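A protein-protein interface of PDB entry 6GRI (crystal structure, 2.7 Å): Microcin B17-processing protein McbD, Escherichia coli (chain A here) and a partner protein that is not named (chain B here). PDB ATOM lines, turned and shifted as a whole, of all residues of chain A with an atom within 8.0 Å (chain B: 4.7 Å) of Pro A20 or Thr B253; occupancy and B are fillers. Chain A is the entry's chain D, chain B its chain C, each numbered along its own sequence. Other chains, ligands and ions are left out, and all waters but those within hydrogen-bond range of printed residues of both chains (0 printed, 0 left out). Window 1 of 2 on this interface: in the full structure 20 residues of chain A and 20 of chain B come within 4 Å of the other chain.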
ATOM      1  N   MET A   1       4.061 -15.430 -10.546  1.00  0.00           N
ATOM      2  CA  MET A   1       2.571 -15.407 -10.416  1.00  0.00           C
ATOM      3  C   MET A   1       2.098 -14.657  -9.163  1.00  0.00           C
ATOM      4  O   MET A   1       2.910 -14.303  -8.303  1.00  0.00           O
ATOM      5  CB  MET A   1       2.025 -16.837 -10.452  1.00  0.00           C
ATOM      6  CG  MET A   1       1.798 -17.346 -11.872  1.00  0.00           C
ATOM      7  SD  MET A   1       1.416 -19.100 -11.964  1.00  0.00           S
ATOM      8  CE  MET A   1       2.916 -19.843 -11.317  1.00  0.00           C
ATOM      9  N   ASN A   3       1.851 -11.784  -7.907  1.00  0.00           N
ATOM     10  CA  ASN A   3       2.540 -10.539  -8.280  1.00  0.00           C
ATOM     11  C   ASN A   3       1.840  -9.255  -7.821  1.00  0.00           C
ATOM     12  O   ASN A   3       1.576  -8.337  -8.629  1.00  0.00           O
ATOM     13  CB  ASN A   3       2.793 -10.518  -9.793  1.00  0.00           C
ATOM     14  CG  ASN A   3       3.758 -11.596 -10.236  1.00  0.00           C
ATOM     15  OD1 ASN A   3       3.419 -12.451 -11.058  1.00  0.00           O
ATOM     16  ND2 ASN A   3       4.970 -11.556  -9.699  1.00  0.00           N
ATOM     17  N   ALA A  17       5.009 -12.790  -4.381  1.00  0.00           N
ATOM     18  CA  ALA A  17       5.051 -13.542  -5.628  1.00  0.00           C
ATOM     19  C   ALA A  17       5.070 -15.039  -5.360  1.00  0.00           C
ATOM     20  O   ALA A  17       5.751 -15.510  -4.461  1.00  0.00           O
ATOM     21  CB  ALA A  17       6.268 -13.147  -6.442  1.00  0.00           C
ATOM     22  N   MET A  18       4.280 -15.765  -6.137  1.00  0.00           N
ATOM     23  CA  MET A  18       4.350 -17.204  -6.225  1.00  0.00           C
ATOM     24  C   MET A  18       5.348 -17.487  -7.322  1.00  0.00           C
ATOM     25  O   MET A  18       5.290 -16.882  -8.377  1.00  0.00           O
ATOM     26  CB  MET A  18       2.979 -17.772  -6.583  1.00  0.00           C
ATOM     27  CG  MET A  18       2.985 -19.219  -7.044  1.00  0.00           C
ATOM     28  SD  MET A  18       1.408 -20.025  -6.740  1.00  0.00           S
ATOM     29  CE  MET A  18       0.276 -19.073  -7.746  1.00  0.00           C
ATOM     30  N   SER A  19       6.260 -18.410  -7.085  1.00  0.00           N
ATOM     31  CA  SER A  19       7.316 -18.677  -8.046  1.00  0.00           C
ATOM     32  C   SER A  19       6.825 -19.574  -9.192  1.00  0.00           C
ATOM     33  O   SER A  19       6.081 -20.524  -8.941  1.00  0.00           O
ATOM     34  CB  SER A  19       8.493 -19.339  -7.361  1.00  0.00           C
ATOM     35  OG  SER A  19       9.561 -19.374  -8.267  1.00  0.00           O
ATOM     36  N   PRO A  20       7.239 -19.292 -10.449  1.00  0.00           N
ATOM     37  CA  PRO A  20       6.892 -20.234 -11.513  1.00  0.00           C
ATOM     38  C   PRO A  20       7.831 -21.406 -11.441  1.00  0.00           C
ATOM     39  O   PRO A  20       8.898 -21.271 -10.870  1.00  0.00           O
ATOM     40  CB  PRO A  20       7.110 -19.435 -12.817  1.00  0.00           C
ATOM     41  CG  PRO A  20       7.674 -18.111 -12.422  1.00  0.00           C
ATOM     42  CD  PRO A  20       8.066 -18.186 -10.966  1.00  0.00           C
ATOM     43  N   LYS A  21       7.426 -22.537 -12.005  1.00  0.00           N
ATOM     44  CA  LYS A  21       8.271 -23.733 -12.065  1.00  0.00           C
ATOM     45  C   LYS A  21       7.940 -24.627 -13.269  1.00  0.00           C
ATOM     46  O   LYS A  21       6.776 -24.788 -13.618  1.00  0.00           O
ATOM     47  CB  LYS A  21       8.121 -24.521 -10.768  1.00  0.00           C
ATOM     48  CG  LYS A  21       6.678 -24.784 -10.371  1.00  0.00           C
ATOM     49  CD  LYS A  21       6.561 -25.998  -9.463  1.00  0.00           C
ATOM     50  CE  LYS A  21       5.189 -26.643  -9.546  1.00  0.00           C
ATOM     51  NZ  LYS A  21       4.219 -26.065  -8.569  1.00  0.00           N
ATOM     52  N   LEU A  22       8.953 -25.217 -13.896  1.00  0.00           N
ATOM     53  CA  LEU A  22       8.700 -26.131 -15.013  1.00  0.00           C
ATOM     54  C   LEU A  22       7.970 -27.408 -14.567  1.00  0.00           C
ATOM     55  O   LEU A  22       6.968 -27.793 -15.157  1.00  0.00           O
ATOM     56  CB  LEU A  22       9.997 -26.523 -15.719  1.00  0.00           C
ATOM     57  CG  LEU A  22      10.900 -25.435 -16.283  1.00  0.00           C
ATOM     58  CD1 LEU A  22      11.954 -26.053 -17.193  1.00  0.00           C
ATOM     59  CD2 LEU A  22      10.103 -24.378 -17.026  1.00  0.00           C
ATOM     60  N   ASN A  23       8.490 -28.049 -13.529  1.00  0.00           N
ATOM     61  CA  ASN A  23       8.075 -29.388 -13.095  1.00  0.00           C
ATOM     62  C   ASN A  23       6.798 -29.294 -12.289  1.00  0.00           C
ATOM     63  O   ASN A  23       6.790 -28.692 -11.223  1.00  0.00           O
ATOM     64  CB  ASN A  23       9.205 -29.983 -12.240  1.00  0.00           C
ATOM     65  CG  ASN A  23       8.915 -31.386 -11.719  1.00  0.00           C
ATOM     66  OD1 ASN A  23       7.796 -31.900 -11.785  1.00  0.00           O
ATOM     67  ND2 ASN A  23       9.956 -32.009 -11.173  1.00  0.00           N
ATOM     68  N   ARG A  24       5.720 -29.906 -12.768  1.00  0.00           N
ATOM     69  CA  ARG A  24       4.449 -29.838 -12.041  1.00  0.00           C
ATOM     70  C   ARG A  24       4.496 -30.551 -10.683  1.00  0.00           C
ATOM     71  O   ARG A  24       3.727 -30.201  -9.802  1.00  0.00           O
ATOM     72  CB  ARG A  24       3.284 -30.360 -12.891  1.00  0.00           C
ATOM     73  CG  ARG A  24       3.235 -31.865 -13.063  1.00  0.00           C
ATOM     74  CD  ARG A  24       2.092 -32.281 -13.975  1.00  0.00           C
ATOM     75  NE  ARG A  24       1.808 -33.713 -13.843  1.00  0.00           N
ATOM     76  CZ  ARG A  24       1.159 -34.280 -12.819  1.00  0.00           C
ATOM     77  NH1 ARG A  24       0.705 -33.563 -11.790  1.00  0.00           N
ATOM     78  NH2 ARG A  24       0.960 -35.593 -12.822  1.00  0.00           N
ATOM     79  N   PRO A  27       7.422 -28.702  -5.540  1.00  0.00           N
ATOM     80  CA  PRO A  27       6.506 -27.851  -4.779  1.00  0.00           C
ATOM     81  C   PRO A  27       6.471 -26.392  -5.272  1.00  0.00           C
ATOM     82  O   PRO A  27       7.403 -25.930  -5.950  1.00  0.00           O
ATOM     83  CB  PRO A  27       7.038 -27.930  -3.341  1.00  0.00           C
ATOM     84  CG  PRO A  27       8.120 -28.956  -3.359  1.00  0.00           C
ATOM     85  CD  PRO A  27       8.627 -29.025  -4.760  1.00  0.00           C
ATOM     86  N   THR A  28       5.373 -25.710  -4.954  1.00  0.00           N
ATOM     87  CA  THR A  28       5.234 -24.288  -5.175  1.00  0.00           C
ATOM     88  C   THR A  28       5.956 -23.572  -4.035  1.00  0.00           C
ATOM     89  O   THR A  28       5.794 -23.939  -2.882  1.00  0.00           O
ATOM     90  CB  THR A  28       3.753 -23.872  -5.166  1.00  0.00           C
ATOM     91  OG1 THR A  28       3.069 -24.472  -6.273  1.00  0.00           O
ATOM     92  CG2 THR A  28       3.603 -22.368  -5.242  1.00  0.00           C
ATOM     93  N   PHE A  29       6.735 -22.549  -4.382  1.00  0.00           N
ATOM     94  CA  PHE A  29       7.448 -21.694  -3.441  1.00  0.00           C
ATOM     95  C   PHE A  29       6.830 -20.296  -3.562  1.00  0.00           C
ATOM     96  O   PHE A  29       6.918 -19.668  -4.606  1.00  0.00           O
ATOM     97  CB  PHE A  29       8.934 -21.689  -3.818  1.00  0.00           C
ATOM     98  CG  PHE A  29       9.794 -20.814  -2.955  1.00  0.00           C
ATOM     99  CD1 PHE A  29      10.383 -21.316  -1.797  1.00  0.00           C
ATOM    100  CD2 PHE A  29      10.054 -19.488  -3.322  1.00  0.00           C
ATOM    101  CE1 PHE A  29      11.186 -20.505  -1.004  1.00  0.00           C
ATOM    102  CE2 PHE A  29      10.852 -18.668  -2.529  1.00  0.00           C
ATOM    103  CZ  PHE A  29      11.419 -19.179  -1.366  1.00  0.00           C
ATOM    104  N   LEU B   8      13.821 -18.742 -12.004  1.00  0.00           N
ATOM    105  CA  LEU B   8      12.591 -18.022 -12.363  1.00  0.00           C
ATOM    106  C   LEU B   8      12.037 -17.093 -11.267  1.00  0.00           C
ATOM    107  O   LEU B   8      11.293 -16.171 -11.575  1.00  0.00           O
ATOM    108  CB  LEU B   8      11.495 -19.003 -12.785  1.00  0.00           C
ATOM    109  CG  LEU B   8      11.731 -19.796 -14.069  1.00  0.00           C
ATOM    110  CD1 LEU B   8      10.625 -20.833 -14.237  1.00  0.00           C
ATOM    111  CD2 LEU B   8      11.818 -18.866 -15.285  1.00  0.00           C
ATOM    112  N   VAL B   9      12.402 -17.327 -10.005  1.00  0.00           N
ATOM    113  CA  VAL B   9      12.012 -16.440  -8.899  1.00  0.00           C
ATOM    114  C   VAL B   9      12.553 -15.021  -9.144  1.00  0.00           C
ATOM    115  O   VAL B   9      11.924 -14.039  -8.754  1.00  0.00           O
ATOM    116  CB  VAL B   9      12.571 -16.913  -7.531  1.00  0.00           C
ATOM    117  CG1 VAL B   9      12.057 -16.026  -6.400  1.00  0.00           C
ATOM    118  CG2 VAL B   9      12.221 -18.365  -7.224  1.00  0.00           C
ATOM    119  N   THR B  12      10.225 -13.640 -11.957  1.00  0.00           N
ATOM    120  CA  THR B  12       8.891 -13.287 -11.460  1.00  0.00           C
ATOM    121  C   THR B  12       8.790 -11.989 -10.659  1.00  0.00           C
ATOM    122  O   THR B  12       7.696 -11.504 -10.438  1.00  0.00           O
ATOM    123  CB  THR B  12       8.249 -14.430 -10.653  1.00  0.00           C
ATOM    124  OG1 THR B  12       6.828 -14.377 -10.808  1.00  0.00           O
ATOM    125  CG2 THR B  12       8.599 -14.364  -9.148  1.00  0.00           C
ATOM    126  N   ILE B 193       7.248 -22.553 -24.309  1.00  0.00           N
ATOM    127  CA  ILE B 193       7.380 -21.179 -23.855  1.00  0.00           C
ATOM    128  C   ILE B 193       7.194 -21.101 -22.323  1.00  0.00           C
ATOM    129  O   ILE B 193       6.175 -21.537 -21.783  1.00  0.00           O
ATOM    130  CB  ILE B 193       6.385 -20.237 -24.573  1.00  0.00           C
ATOM    131  CG1 ILE B 193       6.522 -18.806 -24.044  1.00  0.00           C
ATOM    132  CG2 ILE B 193       4.923 -20.665 -24.411  1.00  0.00           C
ATOM    133  CD1 ILE B 193       6.030 -17.756 -25.006  1.00  0.00           C
ATOM    134  N   ILE B 194       8.184 -20.548 -21.630  1.00  0.00           N
ATOM    135  CA  ILE B 194       8.013 -20.161 -20.242  1.00  0.00           C
ATOM    136  C   ILE B 194       7.437 -18.762 -20.327  1.00  0.00           C
ATOM    137  O   ILE B 194       8.138 -17.832 -20.710  1.00  0.00           O
ATOM    138  CB  ILE B 194       9.352 -20.177 -19.462  1.00  0.00           C
ATOM    139  CG1 ILE B 194       9.959 -21.580 -19.481  1.00  0.00           C
ATOM    140  CG2 ILE B 194       9.152 -19.735 -18.013  1.00  0.00           C
ATOM    141  CD1 ILE B 194      11.376 -21.610 -18.971  1.00  0.00           C
ATOM    142  N   PHE B 195       6.161 -18.621 -19.976  1.00  0.00           N
ATOM    143  CA  PHE B 195       5.418 -17.370 -20.190  1.00  0.00           C
ATOM    144  C   PHE B 195       6.086 -16.179 -19.505  1.00  0.00           C
ATOM    145  O   PHE B 195       6.359 -15.160 -20.155  1.00  0.00           O
ATOM    146  CB  PHE B 195       3.968 -17.484 -19.695  1.00  0.00           C
ATOM    147  CG  PHE B 195       3.097 -18.413 -20.511  1.00  0.00           C
ATOM    148  CD1 PHE B 195       2.735 -18.091 -21.812  1.00  0.00           C
ATOM    149  CD2 PHE B 195       2.584 -19.584 -19.954  1.00  0.00           C
ATOM    150  CE1 PHE B 195       1.903 -18.929 -22.557  1.00  0.00           C
ATOM    151  CE2 PHE B 195       1.765 -20.429 -20.698  1.00  0.00           C
ATOM    152  CZ  PHE B 195       1.427 -20.101 -22.001  1.00  0.00           C
ATOM    153  N   GLU B 196       6.364 -16.324 -18.210  1.00  0.00           N
ATOM    154  CA  GLU B 196       6.922 -15.227 -17.402  1.00  0.00           C
ATOM    155  C   GLU B 196       8.305 -14.740 -17.863  1.00  0.00           C
ATOM    156  O   GLU B 196       8.605 -13.548 -17.763  1.00  0.00           O
ATOM    157  CB  GLU B 196       6.942 -15.598 -15.915  1.00  0.00           C
ATOM    158  CG  GLU B 196       5.538 -15.747 -15.319  1.00  0.00           C
ATOM    159  CD  GLU B 196       5.456 -15.416 -13.833  1.00  0.00           C
ATOM    160  OE1 GLU B 196       6.091 -14.445 -13.374  1.00  0.00           O
ATOM    161  OE2 GLU B 196       4.729 -16.134 -13.116  1.00  0.00           O
ATOM    162  N   ASP B 250       4.053 -27.954 -15.623  1.00  0.00           N
ATOM    163  CA  ASP B 250       3.050 -27.125 -14.977  1.00  0.00           C
ATOM    164  C   ASP B 250       2.597 -26.081 -15.998  1.00  0.00           C
ATOM    165  O   ASP B 250       3.368 -25.219 -16.412  1.00  0.00           O
ATOM    166  CB  ASP B 250       3.650 -26.439 -13.754  1.00  0.00           C
ATOM    167  CG  ASP B 250       2.604 -25.979 -12.775  1.00  0.00           C
ATOM    168  OD1 ASP B 250       1.472 -25.613 -13.176  1.00  0.00           O
ATOM    169  OD2 ASP B 250       2.906 -25.991 -11.569  1.00  0.00           O
ATOM    170  N   GLN B 251       1.338 -26.158 -16.402  1.00  0.00           N
ATOM    171  CA  GLN B 251       0.819 -25.312 -17.493  1.00  0.00           C
ATOM    172  C   GLN B 251       0.666 -23.848 -17.092  1.00  0.00           C
ATOM    173  O   GLN B 251       0.629 -22.975 -17.961  1.00  0.00           O
ATOM    174  CB  GLN B 251      -0.493 -25.876 -18.029  1.00  0.00           C
ATOM    175  CG  GLN B 251      -0.331 -27.277 -18.594  1.00  0.00           C
ATOM    176  CD  GLN B 251      -1.654 -27.911 -18.912  1.00  0.00           C
ATOM    177  OE1 GLN B 251      -2.424 -27.380 -19.714  1.00  0.00           O
ATOM    178  NE2 GLN B 251      -1.931 -29.052 -18.292  1.00  0.00           N
ATOM    179  N   ARG B 252       0.614 -23.592 -15.780  1.00  0.00           N
ATOM    180  CA  ARG B 252       0.621 -22.233 -15.222  1.00  0.00           C
ATOM    181  C   ARG B 252       1.910 -21.461 -15.510  1.00  0.00           C
ATOM    182  O   ARG B 252       1.923 -20.234 -15.441  1.00  0.00           O
ATOM    183  CB  ARG B 252       0.451 -22.282 -13.709  1.00  0.00           C
ATOM    184  CG  ARG B 252      -0.852 -22.869 -13.205  1.00  0.00           C
ATOM    185  CD  ARG B 252      -0.809 -23.032 -11.695  1.00  0.00           C
ATOM    186  NE  ARG B 252       0.088 -24.112 -11.272  1.00  0.00           N
ATOM    187  CZ  ARG B 252       0.223 -24.535 -10.014  1.00  0.00           C
ATOM    188  NH1 ARG B 252      -0.490 -23.987  -9.030  1.00  0.00           N
ATOM    189  NH2 ARG B 252       1.060 -25.524  -9.735  1.00  0.00           N
ATOM    190  N   THR B 253       2.988 -22.196 -15.788  1.00  0.00           N
ATOM    191  CA  THR B 253       4.320 -21.647 -16.029  1.00  0.00           C
ATOM    192  C   THR B 253       4.816 -21.815 -17.470  1.00  0.00           C
ATOM    193  O   THR B 253       5.463 -20.903 -17.998  1.00  0.00           O
ATOM    194  CB  THR B 253       5.307 -22.304 -15.038  1.00  0.00           C
ATOM    195  OG1 THR B 253       4.998 -21.841 -13.719  1.00  0.00           O
ATOM    196  CG2 THR B 253       6.752 -21.967 -15.343  1.00  0.00           C
ATOM    197  N   VAL B 254       4.510 -22.957 -18.088  1.00  0.00           N
ATOM    198  CA  VAL B 254       5.126 -23.372 -19.342  1.00  0.00           C
ATOM    199  C   VAL B 254       4.159 -24.173 -20.227  1.00  0.00           C
ATOM    200  O   VAL B 254       3.354 -24.940 -19.738  1.00  0.00           O
ATOM    201  CB  VAL B 254       6.413 -24.193 -19.065  1.00  0.00           C
ATOM    202  CG1 VAL B 254       6.128 -25.404 -18.186  1.00  0.00           C
ATOM    203  CG2 VAL B 254       7.078 -24.637 -20.357  1.00  0.00           C
ATOM    204  N   ALA B 255       4.263 -24.002 -21.540  1.00  0.00           N
ATOM    205  CA  ALA B 255       3.310 -24.591 -22.482  1.00  0.00           C
ATOM    206  C   ALA B 255       3.995 -25.033 -23.780  1.00  0.00           C
ATOM    207  O   ALA B 255       4.871 -24.324 -24.278  1.00  0.00           O
ATOM    208  CB  ALA B 255       2.195 -23.590 -22.784  1.00  0.00           C
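The side-chain hydroxyl (OG1) of Thr B12 lies within hydrogen-bond range of the backbone NH (N) of Met A1 (3.0 Å). The side-chain amide nitrogen (ND2) of Asn A3 lies within hydrogen-bond range of the backbone carbonyl oxygen (O) of Thr B12 (2.8 Å). N of Met A1 is in hydrogen-bond range of OE2 of Glu B196 (2.7 Å). The side-chain carboxylate of Asp B250 lies within salt-bridge range of the side-chain amino group of Lys A21 (3.3 Å). The backbone NH (N) of Asp B250 is in hydrogen-bond range of the backbone carbonyl oxygen (O) of Leu A22 (3.0 Å). OG1 of Thr B253 lies within hydrogen-bond range of N of Lys A21 (3.1 Å). The side-chain sulfur (SD) of Met A1 lies close to the backbone carbonyl oxygen (O) of Arg B252, 3.7 Å away. NH2 of Arg B252 lies close to NZ of Lys A21 (3.4 Å).
The backbone NH (N) of Phe B195 sits at hydrogen-bond distance from the backbone carbonyl oxygen (O) of Thr B253 (3.1 Å). OD2 of Asp B250 is in salt-bridge range of NH2 of Arg B252 (2.6 Å). OD1 of Asn A3 sits at hydrogen-bond distance from N of Met A1 (3.1 Å). The backbone carbonyl oxygen of Met A18 sits at hydrogen-bond distance from the backbone NH of Met A1 (2.9 Å). The backbone NH (N) of Ser A19 lies within hydrogen-bond range of the backbone carbonyl oxygen (O) of Phe A29. The side-chain amino group of Lys A21 lies within hydrogen-bond range of the side-chain hydroxyl of Thr A28, at 3.0 Å.
Among the printed residues, pairs that only touch across the chains: Met A1 with Thr B253 (3.8 Å), Ala A17 with Thr B12 (3.8 Å), Met A18 with Thr B12 (3.8 Å), Ser A19 with Val B9 (3.0 Å), Pro A20 with Leu B8 (3.8 Å), Pro A20 with Thr B12 (3.8 Å), Pro A20 with Glu B196 (3.6 Å), Pro A20 with Thr B253 (3.3 Å), Leu A22 with Ile B194 (3.6 Å), Leu A22 with Val B254 (3.9 Å) and Arg A24 with Asp B250 (3.7 Å).
Of the printed residues of chain B, Ser A19 touches Val B9. Pro A20 touches four residues of chain B. Printed residues of chain B within 4 Å of Lys A21: Asp B250, Arg B252 and Thr B253. Ile B193 touches none of the printed residues of chain A. Printed residues of chain A within 4 Å of Asp B250: Lys A21, Leu A22 and Arg A24. Thr B253 touches three residues of chain A. The nearest residue of chain B that does not touch Pro A20 is Val B9 (4.5 Å).
Printed residues of chain A that touch a printed residue of chain B: Met A1, Asn A3, Ala A17, Met A18, Ser A19, Pro A20, Lys A21, Leu A22 and Arg A24. Hydrophobic or aromatic side chains of chain A that line the printed part of chain B: Met A1, Ala A17, Pro A20 and Leu A22. Along chain A the printed residues that touch a printed residue of chain B span positions 1 to 24. Of the 13 printed residues of chain B, 9 touch a printed residue of chain A.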
